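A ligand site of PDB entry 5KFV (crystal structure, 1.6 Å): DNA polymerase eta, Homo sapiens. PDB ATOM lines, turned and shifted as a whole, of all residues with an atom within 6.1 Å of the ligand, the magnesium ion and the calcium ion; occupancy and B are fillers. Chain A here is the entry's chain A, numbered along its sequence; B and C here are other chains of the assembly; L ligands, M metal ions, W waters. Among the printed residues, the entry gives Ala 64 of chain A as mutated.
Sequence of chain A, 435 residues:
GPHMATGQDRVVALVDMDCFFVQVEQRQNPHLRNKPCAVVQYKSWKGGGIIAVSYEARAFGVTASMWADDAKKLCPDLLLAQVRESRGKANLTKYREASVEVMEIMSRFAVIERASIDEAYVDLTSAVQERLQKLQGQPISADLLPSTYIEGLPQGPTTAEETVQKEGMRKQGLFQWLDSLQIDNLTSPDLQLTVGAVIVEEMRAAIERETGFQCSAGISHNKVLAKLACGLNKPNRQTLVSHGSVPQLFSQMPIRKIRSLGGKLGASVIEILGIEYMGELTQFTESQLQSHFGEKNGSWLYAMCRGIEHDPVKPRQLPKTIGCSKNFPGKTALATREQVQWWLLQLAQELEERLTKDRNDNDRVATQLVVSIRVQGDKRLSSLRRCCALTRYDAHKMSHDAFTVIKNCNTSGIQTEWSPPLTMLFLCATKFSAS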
ATOM      1  N   ASP A  16      26.140  24.671  -4.121  1.00  0.00           N
ATOM      2  CA  ASP A  16      25.654  23.327  -3.918  1.00  0.00           C
ATOM      3  C   ASP A  16      24.143  23.243  -3.693  1.00  0.00           C
ATOM      4  O   ASP A  16      23.660  23.771  -2.779  1.00  0.00           O
ATOM      5  CB  ASP A  16      26.316  22.669  -2.742  1.00  0.00           C
ATOM      6  CG  ASP A  16      25.797  21.284  -2.484  1.00  0.00           C
ATOM      7  OD1 ASP A  16      24.805  21.221  -1.941  1.00  0.00           O
ATOM      8  OD2 ASP A  16      26.342  20.369  -2.904  1.00  0.00           O
ATOM      9  N   MET A  17      23.480  22.476  -4.519  1.00  0.00           N
ATOM     10  CA  MET A  17      22.044  22.428  -4.369  1.00  0.00           C
ATOM     11  C   MET A  17      21.611  21.844  -3.009  1.00  0.00           C
ATOM     12  O   MET A  17      22.232  20.989  -2.552  1.00  0.00           O
ATOM     13  CB  MET A  17      21.424  21.639  -5.502  1.00  0.00           C
ATOM     14  CG  MET A  17      21.834  22.092  -6.873  1.00  0.00           C
ATOM     15  SD  MET A  17      21.525  23.852  -7.224  1.00  0.00           S
ATOM     16  CE  MET A  17      19.758  23.900  -7.236  1.00  0.00           C
ATOM     17  N   ASP A  18      20.555  22.345  -2.411  1.00  0.00           N
ATOM     18  CA  ASP A  18      20.056  21.778  -1.176  1.00  0.00           C
ATOM     19  C   ASP A  18      19.251  20.518  -1.481  1.00  0.00           C
ATOM     20  O   ASP A  18      18.509  20.505  -2.376  1.00  0.00           O
ATOM     21  CB  ASP A  18      19.130  22.731  -0.483  1.00  0.00           C
ATOM     22  CG  ASP A  18      19.812  24.012  -0.036  1.00  0.00           C
ATOM     23  OD1 ASP A  18      20.983  24.013   0.207  1.00  0.00           O
ATOM     24  OD2 ASP A  18      19.130  24.970   0.082  1.00  0.00           O
ATOM     25  N   CYS A  19      19.531  19.475  -0.728  1.00  0.00           N
ATOM     26  CA  CYS A  19      18.793  18.208  -0.798  1.00  0.00           C
ATOM     27  C   CYS A  19      18.364  17.838  -2.219  1.00  0.00           C
ATOM     28  O   CYS A  19      17.262  17.720  -2.463  1.00  0.00           O
ATOM     29  CB  CYS A  19      17.729  17.990   0.265  1.00  0.00           C
ATOM     30  SG  CYS A  19      16.455  19.206   0.307  1.00  0.00           S
ATOM     31  N   PHE A  20      19.322  17.785  -3.132  1.00  0.00           N
ATOM     32  CA  PHE A  20      18.992  17.977  -4.525  1.00  0.00           C
ATOM     33  C   PHE A  20      17.993  16.988  -5.138  1.00  0.00           C
ATOM     34  O   PHE A  20      17.048  17.411  -5.645  1.00  0.00           O
ATOM     35  CB  PHE A  20      20.276  17.897  -5.366  1.00  0.00           C
ATOM     36  CG  PHE A  20      20.092  18.174  -6.819  1.00  0.00           C
ATOM     37  CD1 PHE A  20      19.375  19.248  -7.232  1.00  0.00           C
ATOM     38  CD2 PHE A  20      20.623  17.370  -7.765  1.00  0.00           C
ATOM     39  CE1 PHE A  20      19.211  19.505  -8.555  1.00  0.00           C
ATOM     40  CE2 PHE A  20      20.440  17.624  -9.094  1.00  0.00           C
ATOM     41  CZ  PHE A  20      19.752  18.709  -9.473  1.00  0.00           C
ATOM     42  N   PHE A  21      18.163  15.702  -4.976  1.00  0.00           N
ATOM     43  CA  PHE A  21      17.227  14.790  -5.625  1.00  0.00           C
ATOM     44  C   PHE A  21      15.836  14.961  -5.018  1.00  0.00           C
ATOM     45  O   PHE A  21      14.843  14.769  -5.694  1.00  0.00           O
ATOM     46  CB  PHE A  21      17.631  13.306  -5.513  1.00  0.00           C
ATOM     47  CG  PHE A  21      18.816  12.897  -6.338  1.00  0.00           C
ATOM     48  CD1 PHE A  21      19.668  13.821  -6.938  1.00  0.00           C
ATOM     49  CD2 PHE A  21      19.096  11.548  -6.497  1.00  0.00           C
ATOM     50  CE1 PHE A  21      20.771  13.393  -7.675  1.00  0.00           C
ATOM     51  CE2 PHE A  21      20.190  11.118  -7.237  1.00  0.00           C
ATOM     52  CZ  PHE A  21      21.033  12.045  -7.818  1.00  0.00           C
ATOM     53  N   VAL A  22      15.774  15.313  -3.731  1.00  0.00           N
ATOM     54  CA  VAL A  22      14.486  15.571  -3.100  1.00  0.00           C
ATOM     55  C   VAL A  22      13.801  16.795  -3.743  1.00  0.00           C
ATOM     56  O   VAL A  22      12.607  16.775  -4.030  1.00  0.00           O
ATOM     57  CB  VAL A  22      14.644  15.771  -1.584  1.00  0.00           C
ATOM     58  CG1 VAL A  22      13.410  16.491  -1.010  1.00  0.00           C
ATOM     59  CG2 VAL A  22      14.844  14.424  -0.910  1.00  0.00           C
ATOM     60  N   GLN A  41      16.187   4.319  -3.650  1.00  0.00           N
ATOM     61  CA  GLN A  41      16.312   3.489  -4.836  1.00  0.00           C
ATOM     62  C   GLN A  41      16.139   2.021  -4.464  1.00  0.00           C
ATOM     63  O   GLN A  41      16.635   1.549  -3.448  1.00  0.00           O
ATOM     64  CB  GLN A  41      17.630   3.742  -5.605  1.00  0.00           C
ATOM     65  CG  GLN A  41      18.928   3.618  -4.870  1.00  0.00           C
ATOM     66  CD  GLN A  41      20.162   4.060  -5.697  1.00  0.00           C
ATOM     67  OE1 GLN A  41      20.053   4.592  -6.826  1.00  0.00           O
ATOM     68  NE2 GLN A  41      21.335   3.820  -5.143  1.00  0.00           N
ATOM     69  N   ILE A  51      18.865   7.858  -0.605  1.00  0.00           N
ATOM     70  CA  ILE A  51      20.028   8.586  -1.111  1.00  0.00           C
ATOM     71  C   ILE A  51      19.880  10.105  -1.025  1.00  0.00           C
ATOM     72  O   ILE A  51      20.840  10.820  -1.327  1.00  0.00           O
ATOM     73  CB  ILE A  51      20.364   8.185  -2.554  1.00  0.00           C
ATOM     74  CG1 ILE A  51      19.200   8.465  -3.507  1.00  0.00           C
ATOM     75  CG2 ILE A  51      20.827   6.720  -2.614  1.00  0.00           C
ATOM     76  CD1 ILE A  51      19.605   8.313  -4.987  1.00  0.00           C
ATOM     77  N   ALA A  52      18.720  10.608  -0.588  1.00  0.00           N
ATOM     78  CA  ALA A  52      18.569  12.055  -0.362  1.00  0.00           C
ATOM     79  C   ALA A  52      17.434  12.309   0.619  1.00  0.00           C
ATOM     80  O   ALA A  52      16.445  11.581   0.626  1.00  0.00           O
ATOM     81  CB  ALA A  52      18.323  12.821  -1.694  1.00  0.00           C
ATOM     82  N   VAL A  53      17.571  13.349   1.448  1.00  0.00           N
ATOM     83  CA  VAL A  53      16.663  13.577   2.567  1.00  0.00           C
ATOM     84  C   VAL A  53      16.372  15.046   2.746  1.00  0.00           C
ATOM     85  O   VAL A  53      17.305  15.873   2.805  1.00  0.00           O
ATOM     86  CB  VAL A  53      17.265  13.018   3.906  1.00  0.00           C
ATOM     87  CG1 VAL A  53      16.282  13.139   5.026  1.00  0.00           C
ATOM     88  CG2 VAL A  53      17.727  11.582   3.746  1.00  0.00           C
ATOM     89  N   TYR A  55      15.193  18.521   4.615  1.00  0.00           N
ATOM     90  CA  TYR A  55      15.616  19.019   5.919  1.00  0.00           C
ATOM     91  C   TYR A  55      14.564  18.769   6.998  1.00  0.00           C
ATOM     92  O   TYR A  55      14.917  18.524   8.154  1.00  0.00           O
ATOM     93  CB  TYR A  55      15.985  20.501   5.806  1.00  0.00           C
ATOM     94  CG  TYR A  55      17.348  20.644   5.183  1.00  0.00           C
ATOM     95  CD1 TYR A  55      17.527  20.596   3.814  1.00  0.00           C
ATOM     96  CD2 TYR A  55      18.489  20.736   5.985  1.00  0.00           C
ATOM     97  CE1 TYR A  55      18.799  20.670   3.241  1.00  0.00           C
ATOM     98  CE2 TYR A  55      19.752  20.815   5.432  1.00  0.00           C
ATOM     99  CZ  TYR A  55      19.917  20.784   4.063  1.00  0.00           C
ATOM    100  OH  TYR A  55      21.194  20.862   3.536  1.00  0.00           O
ATOM    101  N   ARG A  58      15.384  15.297   8.069  1.00  0.00           N
ATOM    102  CA  ARG A  58      16.626  15.219   8.810  1.00  0.00           C
ATOM    103  C   ARG A  58      16.415  15.533  10.289  1.00  0.00           C
ATOM    104  O   ARG A  58      17.142  15.031  11.140  1.00  0.00           O
ATOM    105  CB  ARG A  58      17.678  16.155   8.220  1.00  0.00           C
ATOM    106  CG  ARG A  58      17.987  15.848   6.795  1.00  0.00           C
ATOM    107  CD  ARG A  58      19.103  16.726   6.274  1.00  0.00           C
ATOM    108  NE  ARG A  58      19.220  16.590   4.828  1.00  0.00           N
ATOM    109  CZ  ARG A  58      20.203  17.121   4.101  1.00  0.00           C
ATOM    110  NH1 ARG A  58      21.156  17.836   4.698  1.00  0.00           N
ATOM    111  NH2 ARG A  58      20.207  16.927   2.788  1.00  0.00           N
ATOM    112  N   ALA A  64      20.820   9.922   4.508  1.00  0.00           N
ATOM    113  CA  ALA A  64      21.142   9.090   3.349  1.00  0.00           C
ATOM    114  C   ALA A  64      21.955   7.896   3.866  1.00  0.00           C
ATOM    115  O   ALA A  64      22.381   7.916   5.023  1.00  0.00           O
ATOM    116  CB  ALA A  64      21.903   9.885   2.304  1.00  0.00           C
ATOM    117  N   SER A 116      30.211  17.912  -9.075  1.00  0.00           N
ATOM    118  CA  SER A 116      29.340  16.767  -8.826  1.00  0.00           C
ATOM    119  C   SER A 116      28.038  16.994  -9.553  1.00  0.00           C
ATOM    120  O   SER A 116      27.871  18.003 -10.238  1.00  0.00           O
ATOM    121  CB  SER A 116      29.073  16.583  -7.323  1.00  0.00           C
ATOM    122  OG  SER A 116      28.113  17.512  -6.876  1.00  0.00           O
ATOM    123  N   ILE A 117      27.091  16.086  -9.379  1.00  0.00           N
ATOM    124  CA  ILE A 117      25.816  16.223 -10.038  1.00  0.00           C
ATOM    125  C   ILE A 117      25.083  17.495  -9.552  1.00  0.00           C
ATOM    126  O   ILE A 117      24.250  18.043 -10.260  1.00  0.00           O
ATOM    127  CB  ILE A 117      24.935  14.975  -9.821  1.00  0.00           C
ATOM    128  CG1 ILE A 117      23.794  14.957 -10.840  1.00  0.00           C
ATOM    129  CG2 ILE A 117      24.437  14.907  -8.377  1.00  0.00           C
ATOM    130  CD1 ILE A 117      23.037  13.639 -10.887  1.00  0.00           C
ATOM    131  N   ASP A 118      25.419  17.990  -8.363  1.00  0.00           N
ATOM    132  CA  ASP A 118      24.644  19.131  -7.863  1.00  0.00           C
ATOM    133  C   ASP A 118      25.500  20.276  -7.336  1.00  0.00           C
ATOM    134  O   ASP A 118      24.995  21.125  -6.576  1.00  0.00           O
ATOM    135  CB  ASP A 118      23.686  18.660  -6.764  1.00  0.00           C
ATOM    136  CG  ASP A 118      24.320  18.653  -5.387  1.00  0.00           C
ATOM    137  OD1 ASP A 118      25.539  18.331  -5.266  1.00  0.00           O
ATOM    138  OD2 ASP A 118      23.607  19.024  -4.438  1.00  0.00           O
ATOM    139  N   GLU A 119      26.758  20.348  -7.751  1.00  0.00           N
ATOM    140  CA  GLU A 119      27.553  21.485  -7.321  1.00  0.00           C
ATOM    141  C   GLU A 119      28.636  21.853  -8.314  1.00  0.00           C
ATOM    142  O   GLU A 119      29.113  21.023  -9.098  1.00  0.00           O
ATOM    143  CB  GLU A 119      28.171  21.221  -5.958  1.00  0.00           C
ATOM    144  CG  GLU A 119      29.423  20.406  -5.967  1.00  0.00           C
ATOM    145  CD  GLU A 119      29.632  19.715  -4.636  1.00  0.00           C
ATOM    146  OE1 GLU A 119      30.464  20.184  -3.832  1.00  0.00           O
ATOM    147  OE2 GLU A 119      28.944  18.715  -4.375  1.00  0.00           O
ATOM    148  N   LYS A 227      34.116  25.590  -0.526  1.00  0.00           N
ATOM    149  CA  LYS A 227      33.388  24.383  -0.185  1.00  0.00           C
ATOM    150  C   LYS A 227      33.046  24.330   1.300  1.00  0.00           C
ATOM    151  O   LYS A 227      31.908  24.068   1.676  1.00  0.00           O
ATOM    152  CB  LYS A 227      34.193  23.136  -0.587  1.00  0.00           C
ATOM    153  CG  LYS A 227      33.509  21.854  -0.178  1.00  0.00           C
ATOM    154  CD  LYS A 227      32.125  21.731  -0.803  1.00  0.00           C
ATOM    155  CE  LYS A 227      31.487  20.407  -0.436  1.00  0.00           C
ATOM    156  NZ  LYS A 227      30.254  20.116  -1.226  1.00  0.00           N
ATOM    157  N   LYS A 234      23.732  25.891   5.750  1.00  0.00           N
ATOM    158  CA  LYS A 234      22.775  25.244   4.856  1.00  0.00           C
ATOM    159  C   LYS A 234      21.482  25.082   5.626  1.00  0.00           C
ATOM    160  O   LYS A 234      21.510  24.922   6.847  1.00  0.00           O
ATOM    161  CB  LYS A 234      23.282  23.884   4.385  1.00  0.00           C
ATOM    162  CG  LYS A 234      24.103  23.902   3.124  1.00  0.00           C
ATOM    163  CD  LYS A 234      24.100  22.508   2.463  1.00  0.00           C
ATOM    164  CE  LYS A 234      24.563  22.559   1.004  1.00  0.00           C
ATOM    165  NZ  LYS A 234      23.429  22.334   0.025  1.00  0.00           N
ATOM    166  N   PRO A 235      20.335  25.082   4.935  1.00  0.00           N
ATOM    167  CA  PRO A 235      20.070  25.278   3.510  1.00  0.00           C
ATOM    168  C   PRO A 235      19.730  26.711   3.164  1.00  0.00           C
ATOM    169  O   PRO A 235      19.481  27.523   4.047  1.00  0.00           O
ATOM    170  CB  PRO A 235      18.858  24.399   3.264  1.00  0.00           C
ATOM    171  CG  PRO A 235      18.073  24.534   4.546  1.00  0.00           C
ATOM    172  CD  PRO A 235      19.119  24.658   5.643  1.00  0.00           C
ATOM    173  P    DT B   8      32.558  16.335  -1.640  1.00  0.00           P
ATOM    174  OP1  DT B   8      33.441  16.623  -2.782  1.00  0.00           O
ATOM    175  OP2  DT B   8      32.286  17.409  -0.668  1.00  0.00           O
ATOM    176  O5'  DT B   8      31.168  15.822  -2.173  1.00  0.00           O
ATOM    177  C5'  DT B   8      30.799  16.138  -3.444  1.00  0.00           C
ATOM    178  C4'  DT B   8      29.614  15.321  -3.915  1.00  0.00           C
ATOM    179  O4'  DT B   8      29.898  13.922  -4.086  1.00  0.00           O
ATOM    180  C3'  DT B   8      28.285  15.406  -3.161  1.00  0.00           C
ATOM    181  O3'  DT B   8      27.335  16.074  -3.947  1.00  0.00           O
ATOM    182  C2'  DT B   8      27.888  13.949  -2.898  1.00  0.00           C
ATOM    183  C1'  DT B   8      28.702  13.189  -3.928  1.00  0.00           C
ATOM    184  N1   DT B   8      29.047  11.796  -3.504  1.00  0.00           N
ATOM    185  C2   DT B   8      28.625  10.739  -4.284  1.00  0.00           C
ATOM    186  O2   DT B   8      27.983  10.886  -5.309  1.00  0.00           O
ATOM    187  N3   DT B   8      28.976   9.497  -3.815  1.00  0.00           N
ATOM    188  C4   DT B   8      29.687   9.219  -2.667  1.00  0.00           C
ATOM    189  O4   DT B   8      29.968   8.066  -2.324  1.00  0.00           O
ATOM    190  C5   DT B   8      30.094  10.368  -1.897  1.00  0.00           C
ATOM    191  C7   DT B   8      30.882  10.184  -0.632  1.00  0.00           C
ATOM    192  C6   DT B   8      29.760  11.589  -2.345  1.00  0.00           C
ATOM    193  P    DT C   3      24.993  -3.197   3.959  1.00  0.00           P
ATOM    194  OP1  DT C   3      26.338  -3.838   3.952  1.00  0.00           O
ATOM    195  OP2  DT C   3      24.205  -3.110   5.217  1.00  0.00           O
ATOM    196  O5'  DT C   3      25.146  -1.725   3.376  1.00  0.00           O
ATOM    197  C5'  DT C   3      23.991  -0.978   3.070  1.00  0.00           C
ATOM    198  C4'  DT C   3      24.314   0.135   2.089  1.00  0.00           C
ATOM    199  O4'  DT C   3      24.765   1.294   2.821  1.00  0.00           O
ATOM    200  C3'  DT C   3      25.408  -0.212   1.091  1.00  0.00           C
ATOM    201  O3'  DT C   3      24.934  -0.039  -0.254  1.00  0.00           O
ATOM    202  C2'  DT C   3      26.567   0.738   1.439  1.00  0.00           C
ATOM    203  C1'  DT C   3      25.850   1.882   2.163  1.00  0.00           C
ATOM    204  N1   DT C   3      26.687   2.565   3.182  1.00  0.00           N
ATOM    205  C2   DT C   3      26.840   3.931   3.132  1.00  0.00           C
ATOM    206  O2   DT C   3      26.329   4.625   2.262  1.00  0.00           O
ATOM    207  N3   DT C   3      27.623   4.457   4.121  1.00  0.00           N
ATOM    208  C4   DT C   3      28.250   3.765   5.147  1.00  0.00           C
ATOM    209  O4   DT C   3      28.934   4.332   5.999  1.00  0.00           O
ATOM    210  C5   DT C   3      28.040   2.339   5.152  1.00  0.00           C
ATOM    211  C7   DT C   3      28.675   1.495   6.213  1.00  0.00           C
ATOM    212  C6   DT C   3      27.284   1.807   4.180  1.00  0.00           C
ATOM    213  P    DT C   4      25.013  -1.260  -1.296  1.00  0.00           P
ATOM    214  OP1  DT C   4      24.177  -2.381  -0.801  1.00  0.00           O
ATOM    215  OP2  DT C   4      26.461  -1.466  -1.537  1.00  0.00           O
ATOM    216  O5'  DT C   4      24.417  -0.684  -2.660  1.00  0.00           O
ATOM    217  C5'  DT C   4      23.019  -0.748  -2.959  1.00  0.00           C
ATOM    218  C4'  DT C   4      22.706   0.123  -4.173  1.00  0.00           C
ATOM    219  O4'  DT C   4      23.040   1.491  -3.862  1.00  0.00           O
ATOM    220  C3'  DT C   4      23.514  -0.224  -5.423  1.00  0.00           C
ATOM    221  O3'  DT C   4      22.742   0.108  -6.553  1.00  0.00           O
ATOM    222  C2'  DT C   4      24.745   0.704  -5.287  1.00  0.00           C
ATOM    223  C1'  DT C   4      24.081   1.956  -4.710  1.00  0.00           C
ATOM    224  N1   DT C   4      24.937   2.842  -3.888  1.00  0.00           N
ATOM    225  C2   DT C   4      24.717   4.183  -3.973  1.00  0.00           C
ATOM    226  O2   DT C   4      23.895   4.660  -4.730  1.00  0.00           O
ATOM    227  N3   DT C   4      25.494   4.954  -3.165  1.00  0.00           N
ATOM    228  C4   DT C   4      26.450   4.532  -2.275  1.00  0.00           C
ATOM    229  O4   DT C   4      27.085   5.319  -1.592  1.00  0.00           O
ATOM    230  C5   DT C   4      26.631   3.098  -2.206  1.00  0.00           C
ATOM    231  C7   DT C   4      27.659   2.519  -1.273  1.00  0.00           C
ATOM    232  C6   DT C   4      25.872   2.319  -3.000  1.00  0.00           C
ATOM    233  P    DA C   5      23.308  -0.124  -8.040  1.00  0.00           P
ATOM    234  OP1  DA C   5      22.168  -0.630  -8.841  1.00  0.00           O
ATOM    235  OP2  DA C   5      24.580  -0.866  -7.968  1.00  0.00           O
ATOM    236  O5'  DA C   5      23.672   1.345  -8.516  1.00  0.00           O
ATOM    237  C5'  DA C   5      22.634   2.331  -8.685  1.00  0.00           C
ATOM    238  C4'  DA C   5      23.215   3.615  -9.200  1.00  0.00           C
ATOM    239  O4'  DA C   5      23.994   4.242  -8.140  1.00  0.00           O
ATOM    240  C3'  DA C   5      24.165   3.443 -10.378  1.00  0.00           C
ATOM    241  O3'  DA C   5      24.006   4.528 -11.277  1.00  0.00           O
ATOM    242  C2'  DA C   5      25.536   3.489  -9.703  1.00  0.00           C
ATOM    243  C1'  DA C   5      25.278   4.561  -8.650  1.00  0.00           C
ATOM    244  N9   DA C   5      26.234   4.541  -7.547  1.00  0.00           N
ATOM    245  C8   DA C   5      26.789   3.449  -6.951  1.00  0.00           C
ATOM    246  N7   DA C   5      27.611   3.742  -5.962  1.00  0.00           N
ATOM    247  C5   DA C   5      27.577   5.128  -5.901  1.00  0.00           C
ATOM    248  C6   DA C   5      28.223   6.045  -5.059  1.00  0.00           C
ATOM    249  N6   DA C   5      29.066   5.701  -4.083  1.00  0.00           N
ATOM    250  N1   DA C   5      27.977   7.361  -5.268  1.00  0.00           N
ATOM    251  C2   DA C   5      27.122   7.713  -6.245  1.00  0.00           C
ATOM    252  N3   DA C   5      26.450   6.926  -7.090  1.00  0.00           N
ATOM    253  C4   DA C   5      26.736   5.639  -6.860  1.00  0.00           C
HETATM  254  P1  LIG L   1      22.626  18.846   1.025  1.00  0.00           P
HETATM  255  O1  LIG L   1      23.645  19.255   0.003  1.00  0.00           O
HETATM  256  O2  LIG L   1      21.617  19.950   1.268  1.00  0.00           O
HETATM  257  O3  LIG L   1      23.282  18.393   2.334  1.00  0.00           O
HETATM  258  P2  LIG L   1      22.115  16.828  -0.905  1.00  0.00           P
HETATM  259  O4  LIG L   1      22.125  17.816  -2.029  1.00  0.00           O
HETATM  260  O5  LIG L   1      21.057  15.767  -1.080  1.00  0.00           O
HETATM  261  O6  LIG L   1      21.833  17.560   0.498  1.00  0.00           O
HETATM  262  P3  LIG L   1      24.771  16.074  -1.657  1.00  0.00           P
HETATM  263  O7  LIG L   1      25.176  17.447  -2.072  1.00  0.00           O
HETATM  264  O8  LIG L   1      25.846  15.366  -0.866  1.00  0.00           O
HETATM  265  O9  LIG L   1      23.503  16.083  -0.701  1.00  0.00           O
HETATM  266  O10 LIG L   1      24.461  15.153  -2.906  1.00  0.00           O
HETATM  267  C1  LIG L   1      23.742  15.630  -4.001  1.00  0.00           C
HETATM  268  C2  LIG L   1      22.875  14.522  -4.575  1.00  0.00           C
HETATM  269  O11 LIG L   1      23.723  13.504  -5.050  1.00  0.00           O
HETATM  270  C3  LIG L   1      21.998  13.935  -3.571  1.00  0.00           C
HETATM  271  O12 LIG L   1      20.739  14.639  -3.541  1.00  0.00           O
HETATM  272  C4  LIG L   1      21.825  12.532  -4.005  1.00  0.00           C
HETATM  273  C5  LIG L   1      23.126  12.244  -4.683  1.00  0.00           C
HETATM  274  N1  LIG L   1      24.023  11.547  -3.825  1.00  0.00           N
HETATM  275  C6  LIG L   1      24.850  12.051  -2.883  1.00  0.00           C
HETATM  276  N2  LIG L   1      25.550  11.078  -2.305  1.00  0.00           N
HETATM  277  C7  LIG L   1      25.212   9.918  -2.872  1.00  0.00           C
HETATM  278  C8  LIG L   1      25.591   8.589  -2.723  1.00  0.00           C
HETATM  279  N3  LIG L   1      26.554   8.224  -1.738  1.00  0.00           N
HETATM  280  N4  LIG L   1      25.022   7.654  -3.470  1.00  0.00           N
HETATM  281  C9  LIG L   1      24.103   7.926  -4.404  1.00  0.00           C
HETATM  282  N5  LIG L   1      23.718   9.210  -4.600  1.00  0.00           N
HETATM  283  C10 LIG L   1      24.243  10.196  -3.851  1.00  0.00           C
HETATM  284 MG    MG M   1      27.013  18.306  -3.385  1.00  0.00          MG
HETATM  285 CA    CA M   2      23.816  19.288  -2.214  1.00  0.00          CA
HETATM  286  O   HOH W   1      27.846  18.197  -1.314  1.00  0.00           O
HETATM  287  O   HOH W   2      23.419  10.520  -0.692  1.00  0.00           O
HETATM  288  O   HOH W   3      23.969  15.995   3.086  1.00  0.00           O
HETATM  289  O   HOH W   4      26.340  14.583  -5.604  1.00  0.00           O
HETATM  290  O   HOH W   5      22.772   9.010  -7.249  1.00  0.00           O
HETATM  291  O   HOH W   6      25.950  11.475  -6.615  1.00  0.00           O
HETATM  292  O   HOH W   7      27.081  10.838   0.042  1.00  0.00           O
HETATM  293  O   HOH W   8      26.303  19.323   0.713  1.00  0.00           O
HETATM  294  O   HOH W   9      20.107  14.601   1.190  1.00  0.00           O
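N3 of DT 8 of chain B sits close to a nitrogen (N3) of the ligand.
An oxygen (O2) of the ligand sits at hydrogen-bond distance from the side-chain hydroxyl of Tyr 55.
A nitrogen (N3) of the ligand sits at hydrogen-bond distance from O4 of DT 4 of chain C (3.0 Å).
An oxygen (O3) of the ligand is in salt-bridge range of the guanidinium group of Arg 58, 3.2 Å away.
An oxygen (O2) of the ligand lies within hydrogen-bond range of the backbone NH of Cys 19 (2.9 Å).
N of Phe 20 sits at hydrogen-bond distance from O5 of the ligand.
O2 of the ligand is in salt-bridge range of NZ of Lys 234 (3.2 Å).
An oxygen (O12) of the ligand lies within hydrogen-bond range of the backbone NH of Phe 21.
The side-chain amino group (NZ) of Lys 234 lies within hydrogen-bond range of the backbone carbonyl oxygen (O) of Asp 16 (3.2 Å).
The backbone NH of Asp 118 lies close to the side-chain hydroxyl of Ser 116 (3.1 Å).
O3' of DT 8 of chain B lies close to OG of Ser 116 (3.4 Å).
OP2 of DT 8 of chain B is in salt-bridge range of NZ of Lys 227 (3.4 Å).
The backbone carbonyl oxygen of Met 17 lies close to the side-chain amino group of Lys 234, at 3.1 Å.
NH1 of Arg 58 lies within hydrogen-bond range of OH of Tyr 55 (3.2 Å).
O2 of DT 4 of chain C sits at hydrogen-bond distance from the side-chain amide nitrogen of Gln 41 (2.7 Å).
NZ of Lys 234 lies within salt-bridge range of OD1 of Asp 18, at 3.0 Å.
N1 of DA 5 of chain C sits close to N4 of the ligand, 3.5 Å away.
Asp 18 touches the ligand (CA to O2, 3.4 Å).
Ile 51 touches the ligand (O to C4, 3.3 Å).
Ala 52 touches the ligand.
Ile 117 touches the ligand (CG2 to O11, 3.7 Å).
Hydrophobic or aromatic side chains within 4 Å of the ligand: Phe 20, Phe 21, Ile 51, Ala 52, Tyr 55 and Ile 117.
16 residues have an atom within 4 Å of the ligand: Asp 16, Met 17, Asp 18, Cys 19, Phe 20, Phe 21, Ile 51, Ala 52, Tyr 55, Arg 58, Ile 117, Asp 118, Lys 234, DT 8 of chain B, DT 4 of chain C and DA 5 of chain C.
The nearest printed residue that does not touch the ligand is Glu 119 (4.6 Å).
Ser 116 touches the magnesium ion.
Within 4 Å of the magnesium ion: Asp 16, Ser 116, Asp 118, Glu 119 and DT 8 of chain B.
The nearest printed residue that does not touch the magnesium ion is Lys 227 (4.3 Å).
Residues that only touch the calcium ion: Lys 234 (3.8 Å).
The magnesium ion is bound by OE2 of Glu 119 (2.2 Å), OD2 of Asp 16 (2.2 Å), water W1 (2.2 Å), O3' of DT 8 of chain B (2.3 Å), OD1 of Asp 118 (2.4 Å) and O7 of the ligand (2.4 Å).
The magnesium ion has six donor atoms within binding distance.
The calcium ion is bound by OD1 of Asp 16 (2.2 Å).
An oxygen (O1) of the ligand is bound to the calcium ion (2.2 Å).
OD2 of Asp 118 binds the calcium ion (2.2 Å).
The calcium ion is bound by O4 of the ligand, at 2.2 Å.
The calcium ion is bound by O7 of the ligand (2.3 Å).
The backbone carbonyl oxygen (O) of Met 17 binds the calcium ion.
The side-chain carboxylate (OD2) of Asp 16 is bound to the calcium ion (2.8 Å).
Water W1 bridges NZ of Lys 227 and O8 of the ligand.
Water W9 lies within hydrogen-bond range of an oxygen (O5) of the ligand, the guanidinium group (NH2) of Arg 58 and the backbone NH (N) of Val 53.
Water W2 bridges O of Ile 51 (2.7 Å) and N2 of the ligand (2.7 Å).
Water W6 bridges O2 of DT 8 of chain B (2.5 Å) and an oxygen (O11) of the ligand (3.4 Å).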
